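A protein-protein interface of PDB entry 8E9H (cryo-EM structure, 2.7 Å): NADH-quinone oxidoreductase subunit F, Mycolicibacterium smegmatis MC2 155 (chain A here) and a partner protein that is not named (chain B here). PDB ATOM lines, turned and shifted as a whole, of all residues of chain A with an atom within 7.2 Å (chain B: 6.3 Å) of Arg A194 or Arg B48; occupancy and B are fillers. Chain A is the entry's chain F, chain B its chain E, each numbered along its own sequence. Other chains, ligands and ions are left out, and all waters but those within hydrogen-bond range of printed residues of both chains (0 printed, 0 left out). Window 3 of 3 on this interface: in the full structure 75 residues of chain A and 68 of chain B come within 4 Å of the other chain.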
ATOM      1  N   HIS A 173     -16.164 -28.278  22.858  1.00  0.00           N
ATOM      2  CA  HIS A 173     -16.830 -27.574  21.773  1.00  0.00           C
ATOM      3  C   HIS A 173     -16.461 -28.250  20.462  1.00  0.00           C
ATOM      4  O   HIS A 173     -15.280 -28.320  20.108  1.00  0.00           O
ATOM      5  CB  HIS A 173     -16.429 -26.102  21.753  1.00  0.00           C
ATOM      6  CG  HIS A 173     -17.160 -25.292  20.731  1.00  0.00           C
ATOM      7  ND1 HIS A 173     -18.299 -24.576  21.027  1.00  0.00           N
ATOM      8  CD2 HIS A 173     -16.913 -25.082  19.417  1.00  0.00           C
ATOM      9  CE1 HIS A 173     -18.724 -23.961  19.938  1.00  0.00           C
ATOM     10  NE2 HIS A 173     -17.901 -24.251  18.948  1.00  0.00           N
ATOM     11  N   CYS A 181      -9.694 -22.179  11.600  1.00  0.00           N
ATOM     12  CA  CYS A 181     -10.144 -22.081  12.982  1.00  0.00           C
ATOM     13  C   CYS A 181      -9.103 -22.602  13.958  1.00  0.00           C
ATOM     14  O   CYS A 181      -9.189 -22.303  15.153  1.00  0.00           O
ATOM     15  CB  CYS A 181     -11.452 -22.842  13.169  1.00  0.00           C
ATOM     16  SG  CYS A 181     -12.893 -21.957  12.565  1.00  0.00           S
ATOM     17  N   ALA A 186      -8.926 -17.054  15.662  1.00  0.00           N
ATOM     18  CA  ALA A 186      -9.944 -17.647  14.808  1.00  0.00           C
ATOM     19  C   ALA A 186     -10.619 -18.789  15.539  1.00  0.00           C
ATOM     20  O   ALA A 186     -11.834 -18.981  15.430  1.00  0.00           O
ATOM     21  CB  ALA A 186      -9.324 -18.131  13.501  1.00  0.00           C
ATOM     22  N   LEU A 188     -10.934 -18.557  18.704  1.00  0.00           N
ATOM     23  CA  LEU A 188     -11.776 -17.776  19.600  1.00  0.00           C
ATOM     24  C   LEU A 188     -13.004 -17.238  18.882  1.00  0.00           C
ATOM     25  O   LEU A 188     -14.107 -17.251  19.438  1.00  0.00           O
ATOM     26  CB  LEU A 188     -10.965 -16.632  20.203  1.00  0.00           C
ATOM     27  CG  LEU A 188      -9.647 -17.053  20.846  1.00  0.00           C
ATOM     28  CD1 LEU A 188      -8.942 -15.857  21.441  1.00  0.00           C
ATOM     29  CD2 LEU A 188      -9.888 -18.103  21.908  1.00  0.00           C
ATOM     30  N   ASP A 189     -12.840 -16.759  17.649  1.00  0.00           N
ATOM     31  CA  ASP A 189     -13.987 -16.243  16.913  1.00  0.00           C
ATOM     32  C   ASP A 189     -15.015 -17.337  16.663  1.00  0.00           C
ATOM     33  O   ASP A 189     -16.221 -17.103  16.795  1.00  0.00           O
ATOM     34  CB  ASP A 189     -13.530 -15.627  15.595  1.00  0.00           C
ATOM     35  CG  ASP A 189     -13.022 -14.213  15.765  1.00  0.00           C
ATOM     36  OD1 ASP A 189     -12.826 -13.785  16.921  1.00  0.00           O
ATOM     37  OD2 ASP A 189     -12.823 -13.526  14.741  1.00  0.00           O
ATOM     38  N   SER A 190     -14.563 -18.535  16.298  1.00  0.00           N
ATOM     39  CA  SER A 190     -15.494 -19.642  16.118  1.00  0.00           C
ATOM     40  C   SER A 190     -16.140 -20.032  17.441  1.00  0.00           C
ATOM     41  O   SER A 190     -17.324 -20.384  17.479  1.00  0.00           O
ATOM     42  CB  SER A 190     -14.778 -20.834  15.495  1.00  0.00           C
ATOM     43  OG  SER A 190     -13.865 -21.403  16.411  1.00  0.00           O
ATOM     44  N   LEU A 191     -15.381 -19.981  18.536  1.00  0.00           N
ATOM     45  CA  LEU A 191     -15.970 -20.238  19.845  1.00  0.00           C
ATOM     46  C   LEU A 191     -17.059 -19.226  20.159  1.00  0.00           C
ATOM     47  O   LEU A 191     -18.072 -19.565  20.781  1.00  0.00           O
ATOM     48  CB  LEU A 191     -14.897 -20.204  20.928  1.00  0.00           C
ATOM     49  CG  LEU A 191     -14.281 -21.544  21.315  1.00  0.00           C
ATOM     50  CD1 LEU A 191     -13.061 -21.326  22.178  1.00  0.00           C
ATOM     51  CD2 LEU A 191     -15.296 -22.401  22.041  1.00  0.00           C
ATOM     52  N   GLU A 192     -16.865 -17.979  19.747  1.00  0.00           N
ATOM     53  CA  GLU A 192     -17.846 -16.936  20.003  1.00  0.00           C
ATOM     54  C   GLU A 192     -19.018 -16.978  19.039  1.00  0.00           C
ATOM     55  O   GLU A 192     -19.804 -16.027  19.017  1.00  0.00           O
ATOM     56  CB  GLU A 192     -17.170 -15.572  19.927  1.00  0.00           C
ATOM     57  CG  GLU A 192     -16.296 -15.258  21.118  1.00  0.00           C
ATOM     58  CD  GLU A 192     -15.591 -13.927  20.982  1.00  0.00           C
ATOM     59  OE1 GLU A 192     -16.129 -13.037  20.294  1.00  0.00           O
ATOM     60  OE2 GLU A 192     -14.503 -13.768  21.568  1.00  0.00           O
ATOM     61  N   GLY A 193     -19.165 -18.036  18.252  1.00  0.00           N
ATOM     62  CA  GLY A 193     -20.245 -18.089  17.285  1.00  0.00           C
ATOM     63  C   GLY A 193     -20.110 -17.066  16.181  1.00  0.00           C
ATOM     64  O   GLY A 193     -21.096 -16.411  15.824  1.00  0.00           O
ATOM     65  N   ARG A 194     -18.912 -16.903  15.640  1.00  0.00           N
ATOM     66  CA  ARG A 194     -18.647 -16.003  14.531  1.00  0.00           C
ATOM     67  C   ARG A 194     -17.877 -16.747  13.448  1.00  0.00           C
ATOM     68  O   ARG A 194     -17.506 -17.910  13.603  1.00  0.00           O
ATOM     69  CB  ARG A 194     -17.862 -14.777  14.995  1.00  0.00           C
ATOM     70  CG  ARG A 194     -18.383 -14.147  16.262  1.00  0.00           C
ATOM     71  CD  ARG A 194     -17.520 -12.972  16.659  1.00  0.00           C
ATOM     72  NE  ARG A 194     -17.838 -12.486  17.995  1.00  0.00           N
ATOM     73  CZ  ARG A 194     -18.829 -11.650  18.269  1.00  0.00           C
ATOM     74  NH1 ARG A 194     -19.624 -11.184  17.321  1.00  0.00           N
ATOM     75  NH2 ARG A 194     -19.027 -11.271  19.528  1.00  0.00           N
ATOM     76  N   ARG A 195     -17.638 -16.059  12.338  1.00  0.00           N
ATOM     77  CA  ARG A 195     -16.791 -16.620  11.300  1.00  0.00           C
ATOM     78  C   ARG A 195     -15.393 -16.851  11.852  1.00  0.00           C
ATOM     79  O   ARG A 195     -14.825 -15.996  12.532  1.00  0.00           O
ATOM     80  CB  ARG A 195     -16.733 -15.684  10.097  1.00  0.00           C
ATOM     81  CG  ARG A 195     -18.060 -15.482   9.407  1.00  0.00           C
ATOM     82  CD  ARG A 195     -17.984 -14.334   8.427  1.00  0.00           C
ATOM     83  NE  ARG A 195     -17.024 -14.592   7.364  1.00  0.00           N
ATOM     84  CZ  ARG A 195     -17.232 -15.421   6.351  1.00  0.00           C
ATOM     85  NH1 ARG A 195     -18.363 -16.097   6.234  1.00  0.00           N
ATOM     86  NH2 ARG A 195     -16.284 -15.576   5.434  1.00  0.00           N
ATOM     87  N   GLY A 196     -14.834 -18.014  11.550  1.00  0.00           N
ATOM     88  CA  GLY A 196     -13.526 -18.362  12.061  1.00  0.00           C
ATOM     89  C   GLY A 196     -12.409 -17.589  11.395  1.00  0.00           C
ATOM     90  O   GLY A 196     -11.511 -18.186  10.797  1.00  0.00           O
ATOM     91  N   GLN A 197     -12.451 -16.266  11.492  1.00  0.00           N
ATOM     92  CA  GLN A 197     -11.426 -15.462  10.848  1.00  0.00           C
ATOM     93  C   GLN A 197     -10.484 -14.866  11.884  1.00  0.00           C
ATOM     94  O   GLN A 197     -10.927 -14.451  12.957  1.00  0.00           O
ATOM     95  CB  GLN A 197     -12.060 -14.336  10.038  1.00  0.00           C
ATOM     96  CG  GLN A 197     -13.011 -14.820   8.975  1.00  0.00           C
ATOM     97  CD  GLN A 197     -13.279 -13.772   7.926  1.00  0.00           C
ATOM     98  OE1 GLN A 197     -13.304 -12.581   8.220  1.00  0.00           O
ATOM     99  NE2 GLN A 197     -13.478 -14.208   6.693  1.00  0.00           N
ATOM    100  N   ARG A 199      -8.281 -12.462  14.195  1.00  0.00           N
ATOM    101  CA  ARG A 199      -8.506 -11.110  14.674  1.00  0.00           C
ATOM    102  C   ARG A 199      -7.286 -10.240  14.425  1.00  0.00           C
ATOM    103  O   ARG A 199      -6.196 -10.719  14.107  1.00  0.00           O
ATOM    104  CB  ARG A 199      -8.819 -11.092  16.165  1.00  0.00           C
ATOM    105  CG  ARG A 199     -10.074 -11.815  16.560  1.00  0.00           C
ATOM    106  CD  ARG A 199     -10.153 -11.901  18.065  1.00  0.00           C
ATOM    107  NE  ARG A 199     -11.279 -12.706  18.513  1.00  0.00           N
ATOM    108  CZ  ARG A 199     -11.650 -12.821  19.778  1.00  0.00           C
ATOM    109  NH1 ARG A 199     -10.999 -12.204  20.749  1.00  0.00           N
ATOM    110  NH2 ARG A 199     -12.703 -13.573  20.078  1.00  0.00           N
ATOM    111  N   TYR A 211     -14.438 -13.887  24.431  1.00  0.00           N
ATOM    112  CA  TYR A 211     -15.389 -12.910  24.960  1.00  0.00           C
ATOM    113  C   TYR A 211     -14.681 -11.639  25.415  1.00  0.00           C
ATOM    114  O   TYR A 211     -15.121 -10.967  26.348  1.00  0.00           O
ATOM    115  CB  TYR A 211     -16.212 -13.500  26.105  1.00  0.00           C
ATOM    116  CG  TYR A 211     -16.716 -14.892  25.832  1.00  0.00           C
ATOM    117  CD1 TYR A 211     -17.343 -15.199  24.637  1.00  0.00           C
ATOM    118  CD2 TYR A 211     -16.573 -15.898  26.771  1.00  0.00           C
ATOM    119  CE1 TYR A 211     -17.805 -16.468  24.382  1.00  0.00           C
ATOM    120  CE2 TYR A 211     -17.033 -17.172  26.524  1.00  0.00           C
ATOM    121  CZ  TYR A 211     -17.650 -17.450  25.329  1.00  0.00           C
ATOM    122  OH  TYR A 211     -18.109 -18.718  25.077  1.00  0.00           O
ATOM    123  N   ILE B  41     -27.408 -23.946  24.925  1.00  0.00           N
ATOM    124  CA  ILE B  41     -26.994 -22.609  25.332  1.00  0.00           C
ATOM    125  C   ILE B  41     -26.647 -22.582  26.808  1.00  0.00           C
ATOM    126  O   ILE B  41     -25.869 -21.732  27.255  1.00  0.00           O
ATOM    127  CB  ILE B  41     -28.099 -21.590  25.000  1.00  0.00           C
ATOM    128  CG1 ILE B  41     -28.277 -21.473  23.489  1.00  0.00           C
ATOM    129  CG2 ILE B  41     -27.761 -20.240  25.595  1.00  0.00           C
ATOM    130  CD1 ILE B  41     -29.633 -20.964  23.085  1.00  0.00           C
ATOM    131  N   ASP B  46     -21.390 -17.130  27.034  1.00  0.00           N
ATOM    132  CA  ASP B  46     -22.035 -16.199  26.119  1.00  0.00           C
ATOM    133  C   ASP B  46     -22.980 -16.989  25.228  1.00  0.00           C
ATOM    134  O   ASP B  46     -22.596 -18.025  24.677  1.00  0.00           O
ATOM    135  CB  ASP B  46     -20.999 -15.452  25.280  1.00  0.00           C
ATOM    136  CG  ASP B  46     -21.628 -14.468  24.319  1.00  0.00           C
ATOM    137  OD1 ASP B  46     -22.862 -14.298  24.364  1.00  0.00           O
ATOM    138  OD2 ASP B  46     -20.887 -13.865  23.517  1.00  0.00           O
ATOM    139  N   ALA B  47     -24.210 -16.496  25.083  1.00  0.00           N
ATOM    140  CA  ALA B  47     -25.207 -17.232  24.317  1.00  0.00           C
ATOM    141  C   ALA B  47     -24.752 -17.471  22.887  1.00  0.00           C
ATOM    142  O   ALA B  47     -24.874 -18.589  22.375  1.00  0.00           O
ATOM    143  CB  ALA B  47     -26.533 -16.476  24.325  1.00  0.00           C
ATOM    144  N   ARG B  48     -24.208 -16.446  22.229  1.00  0.00           N
ATOM    145  CA  ARG B  48     -23.807 -16.608  20.838  1.00  0.00           C
ATOM    146  C   ARG B  48     -22.772 -17.709  20.680  1.00  0.00           C
ATOM    147  O   ARG B  48     -22.641 -18.287  19.596  1.00  0.00           O
ATOM    148  CB  ARG B  48     -23.259 -15.298  20.283  1.00  0.00           C
ATOM    149  CG  ARG B  48     -23.064 -15.333  18.784  1.00  0.00           C
ATOM    150  CD  ARG B  48     -22.392 -14.088  18.268  1.00  0.00           C
ATOM    151  NE  ARG B  48     -22.089 -14.214  16.847  1.00  0.00           N
ATOM    152  CZ  ARG B  48     -22.294 -13.271  15.939  1.00  0.00           C
ATOM    153  NH1 ARG B  48     -22.793 -12.090  16.261  1.00  0.00           N
ATOM    154  NH2 ARG B  48     -21.986 -13.520  14.669  1.00  0.00           N
ATOM    155  N   SER B  49     -22.039 -18.025  21.746  1.00  0.00           N
ATOM    156  CA  SER B  49     -21.037 -19.076  21.661  1.00  0.00           C
ATOM    157  C   SER B  49     -21.647 -20.407  21.261  1.00  0.00           C
ATOM    158  O   SER B  49     -20.929 -21.288  20.778  1.00  0.00           O
ATOM    159  CB  SER B  49     -20.315 -19.216  22.998  1.00  0.00           C
ATOM    160  OG  SER B  49     -19.178 -20.044  22.874  1.00  0.00           O
ATOM    161  N   ALA B  50     -22.955 -20.573  21.449  1.00  0.00           N
ATOM    162  CA  ALA B  50     -23.618 -21.821  21.106  1.00  0.00           C
ATOM    163  C   ALA B  50     -24.007 -21.901  19.639  1.00  0.00           C
ATOM    164  O   ALA B  50     -24.611 -22.899  19.236  1.00  0.00           O
ATOM    165  CB  ALA B  50     -24.865 -21.996  21.968  1.00  0.00           C
ATOM    166  N   LEU B  51     -23.680 -20.890  18.834  1.00  0.00           N
ATOM    167  CA  LEU B  51     -24.197 -20.850  17.471  1.00  0.00           C
ATOM    168  C   LEU B  51     -23.744 -22.058  16.663  1.00  0.00           C
ATOM    169  O   LEU B  51     -24.545 -22.665  15.946  1.00  0.00           O
ATOM    170  CB  LEU B  51     -23.767 -19.560  16.781  1.00  0.00           C
ATOM    171  CG  LEU B  51     -24.197 -19.442  15.320  1.00  0.00           C
ATOM    172  CD1 LEU B  51     -25.679 -19.691  15.165  1.00  0.00           C
ATOM    173  CD2 LEU B  51     -23.844 -18.075  14.788  1.00  0.00           C
ATOM    174  N   LEU B  52     -22.466 -22.420  16.752  1.00  0.00           N
ATOM    175  CA  LEU B  52     -21.994 -23.568  15.982  1.00  0.00           C
ATOM    176  C   LEU B  52     -22.723 -24.843  16.362  1.00  0.00           C
ATOM    177  O   LEU B  52     -23.238 -25.527  15.462  1.00  0.00           O
ATOM    178  CB  LEU B  52     -20.481 -23.723  16.152  1.00  0.00           C
ATOM    179  CG  LEU B  52     -19.652 -23.099  15.035  1.00  0.00           C
ATOM    180  CD1 LEU B  52     -19.816 -21.596  15.044  1.00  0.00           C
ATOM    181  CD2 LEU B  52     -18.195 -23.479  15.177  1.00  0.00           C
ATOM    182  N   LEU B  77     -30.558 -16.976  19.326  1.00  0.00           N
ATOM    183  CA  LEU B  77     -29.421 -16.174  19.752  1.00  0.00           C
ATOM    184  C   LEU B  77     -29.642 -14.682  19.569  1.00  0.00           C
ATOM    185  O   LEU B  77     -28.724 -13.898  19.823  1.00  0.00           O
ATOM    186  CB  LEU B  77     -28.167 -16.606  18.991  1.00  0.00           C
ATOM    187  CG  LEU B  77     -27.374 -17.734  19.649  1.00  0.00           C
ATOM    188  CD1 LEU B  77     -28.294 -18.818  20.178  1.00  0.00           C
ATOM    189  CD2 LEU B  77     -26.390 -18.316  18.662  1.00  0.00           C
ATOM    190  N   LEU B  79     -29.735 -13.008  16.951  1.00  0.00           N
ATOM    191  CA  LEU B  79     -29.001 -12.484  15.813  1.00  0.00           C
ATOM    192  C   LEU B  79     -29.938 -12.283  14.631  1.00  0.00           C
ATOM    193  O   LEU B  79     -31.067 -12.771  14.611  1.00  0.00           O
ATOM    194  CB  LEU B  79     -27.875 -13.434  15.416  1.00  0.00           C
ATOM    195  CG  LEU B  79     -26.952 -13.885  16.542  1.00  0.00           C
ATOM    196  CD1 LEU B  79     -25.973 -14.913  16.021  1.00  0.00           C
ATOM    197  CD2 LEU B  79     -26.225 -12.703  17.146  1.00  0.00           C
ATOM    198  N   GLU B  83     -26.340 -12.629  10.025  1.00  0.00           N
ATOM    199  CA  GLU B  83     -25.189 -13.048  10.818  1.00  0.00           C
ATOM    200  C   GLU B  83     -25.119 -14.565  10.913  1.00  0.00           C
ATOM    201  O   GLU B  83     -24.041 -15.162  10.776  1.00  0.00           O
ATOM    202  CB  GLU B  83     -25.268 -12.427  12.210  1.00  0.00           C
ATOM    203  CG  GLU B  83     -25.214 -10.912  12.204  1.00  0.00           C
ATOM    204  CD  GLU B  83     -25.291 -10.318  13.595  1.00  0.00           C
ATOM    205  OE1 GLU B  83     -26.413 -10.195  14.127  1.00  0.00           O
ATOM    206  OE2 GLU B  83     -24.232  -9.971  14.156  1.00  0.00           O
ATOM    207  N   VAL B  84     -26.262 -15.207  11.143  1.00  0.00           N
ATOM    208  CA  VAL B  84     -26.279 -16.658  11.234  1.00  0.00           C
ATOM    209  C   VAL B  84     -25.851 -17.273   9.913  1.00  0.00           C
ATOM    210  O   VAL B  84     -25.105 -18.254   9.888  1.00  0.00           O
ATOM    211  CB  VAL B  84     -27.670 -17.149  11.660  1.00  0.00           C
ATOM    212  CG1 VAL B  84     -27.715 -18.661  11.664  1.00  0.00           C
ATOM    213  CG2 VAL B  84     -28.020 -16.601  13.023  1.00  0.00           C
ATOM    214  N   VAL B  87     -22.084 -17.031   9.527  1.00  0.00           N
ATOM    215  CA  VAL B  87     -21.397 -18.063  10.297  1.00  0.00           C
ATOM    216  C   VAL B  87     -21.561 -19.421   9.629  1.00  0.00           C
ATOM    217  O   VAL B  87     -20.604 -20.194   9.513  1.00  0.00           O
ATOM    218  CB  VAL B  87     -21.913 -18.083  11.743  1.00  0.00           C
ATOM    219  CG1 VAL B  87     -21.277 -19.225  12.504  1.00  0.00           C
ATOM    220  CG2 VAL B  87     -21.619 -16.761  12.414  1.00  0.00           C
ATOM    221  N   PHE B  90     -19.639 -20.321   6.360  1.00  0.00           N
ATOM    222  CA  PHE B  90     -18.192 -20.298   6.494  1.00  0.00           C
ATOM    223  C   PHE B  90     -17.607 -21.685   6.703  1.00  0.00           C
ATOM    224  O   PHE B  90     -16.470 -21.938   6.294  1.00  0.00           O
ATOM    225  CB  PHE B  90     -17.796 -19.393   7.657  1.00  0.00           C
ATOM    226  CG  PHE B  90     -16.322 -19.241   7.824  1.00  0.00           C
ATOM    227  CD1 PHE B  90     -15.617 -18.352   7.043  1.00  0.00           C
ATOM    228  CD2 PHE B  90     -15.640 -19.982   8.765  1.00  0.00           C
ATOM    229  CE1 PHE B  90     -14.263 -18.205   7.197  1.00  0.00           C
ATOM    230  CE2 PHE B  90     -14.284 -19.839   8.921  1.00  0.00           C
ATOM    231  CZ  PHE B  90     -13.595 -18.950   8.137  1.00  0.00           C
ATOM    232  N   TYR B  91     -18.350 -22.589   7.327  1.00  0.00           N
ATOM    233  CA  TYR B  91     -17.836 -23.898   7.693  1.00  0.00           C
ATOM    234  C   TYR B  91     -18.319 -24.955   6.713  1.00  0.00           C
ATOM    235  O   TYR B  91     -19.457 -24.909   6.241  1.00  0.00           O
ATOM    236  CB  TYR B  91     -18.260 -24.261   9.112  1.00  0.00           C
ATOM    237  CG  TYR B  91     -17.801 -23.255  10.134  1.00  0.00           C
ATOM    238  CD1 TYR B  91     -18.577 -22.157  10.451  1.00  0.00           C
ATOM    239  CD2 TYR B  91     -16.584 -23.400  10.773  1.00  0.00           C
ATOM    240  CE1 TYR B  91     -18.158 -21.237  11.380  1.00  0.00           C
ATOM    241  CE2 TYR B  91     -16.158 -22.486  11.701  1.00  0.00           C
ATOM    242  CZ  TYR B  91     -16.948 -21.406  12.001  1.00  0.00           C
ATOM    243  OH  TYR B  91     -16.522 -20.491  12.930  1.00  0.00           O
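Among the printed residues, merely in contact across the chains: His A173 with Ser B49, His A173 with Leu B52, Cys A181 with Tyr B91, Ser A190 with Leu B52, Ser A190 with Tyr B91, Glu A192 with Arg B48, Glu A192 with Ser B49, Gly A193 with Leu B51, Gly A193 with Val B87, Arg A194 with Val B87, Arg A195 with Phe B90, Arg A195 with Tyr B91, Gly A196 with Phe B90 and Tyr A211 with Asp B46.
Printed residues of chain B that touch a printed residue of chain A: Asp B46, Arg B48, Ser B49, Leu B51, Leu B52, Val B87, Phe B90 and Tyr B91.
Hydrophobic or aromatic side chains of chain B within 4 Å of the printed part of chain A: Leu B51, Leu B52, Val B87, Phe B90 and Tyr B91.
Among the printed residues, no Asp or Glu carboxylate lies within 4 Å of a Lys or Arg side-chain nitrogen of the other chain.
N of Arg B48 lies close to OD1 of Asp B46.
NH1 of Arg B48 lies within salt-bridge range of OE2 of Glu B83.
O of Ala A186 lies within hydrogen-bond range of OG of Ser A190 (3.3 Å).
O of Asp A189 lies within hydrogen-bond range of N of Arg A194.
The side-chain carboxylate of Glu A192 lies within salt-bridge range of the guanidinium group of Arg A199, at 3.5 Å.
The side-chain carboxylate (OE2) of Glu A192 sits at hydrogen-bond distance from the backbone NH (N) of Tyr A211 (2.9 Å).
Of chain B, only Arg B48 (3.5 Å), Val B87 (3.7 Å) and Tyr B91 (2.8 Å) come within 4 Å of Arg A194.
Arg B48 touches three residues of chain A.
No residue of chain A comes within 4 Å of Ala B47.
Printed residues of chain B within 4 Å of Gly A193: Arg B48, Leu B51 and Val B87.
Of the printed residues of chain B, Tyr A211 touches Asp B46 (3.5 Å) and Ser B49 (2.8 Å).
Of the printed residues of chain A, Tyr B91 touches Cys A181, Ser A190, Arg A194, Arg A195 and Gly A196.
Arg A199 touches none of the printed residues of chain B.
Asp A189 touches none of the printed residues of chain B.
The guanidinium group (NE) of Arg B48 is in hydrogen-bond range of the backbone carbonyl oxygen (O) of Gly A193, at 2.6 Å.
The side-chain hydroxyl (OG) of Ser B49 lies within hydrogen-bond range of the backbone carbonyl oxygen (O) of Leu A191 (2.4 Å).
OG of Ser B49 is in hydrogen-bond range of OH of Tyr A211 (2.8 Å).
The side-chain hydroxyl (OH) of Tyr B91 is in hydrogen-bond range of the backbone carbonyl oxygen (O) of Arg A194 (2.8 Å).
The backbone NH (N) of Gly A196 is in hydrogen-bond range of the side-chain hydroxyl (OH) of Tyr B91.
The guanidinium group (NH1) of Arg A194 sits close to the guanidinium group (NH1) of Arg B48, at 3.5 Å.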
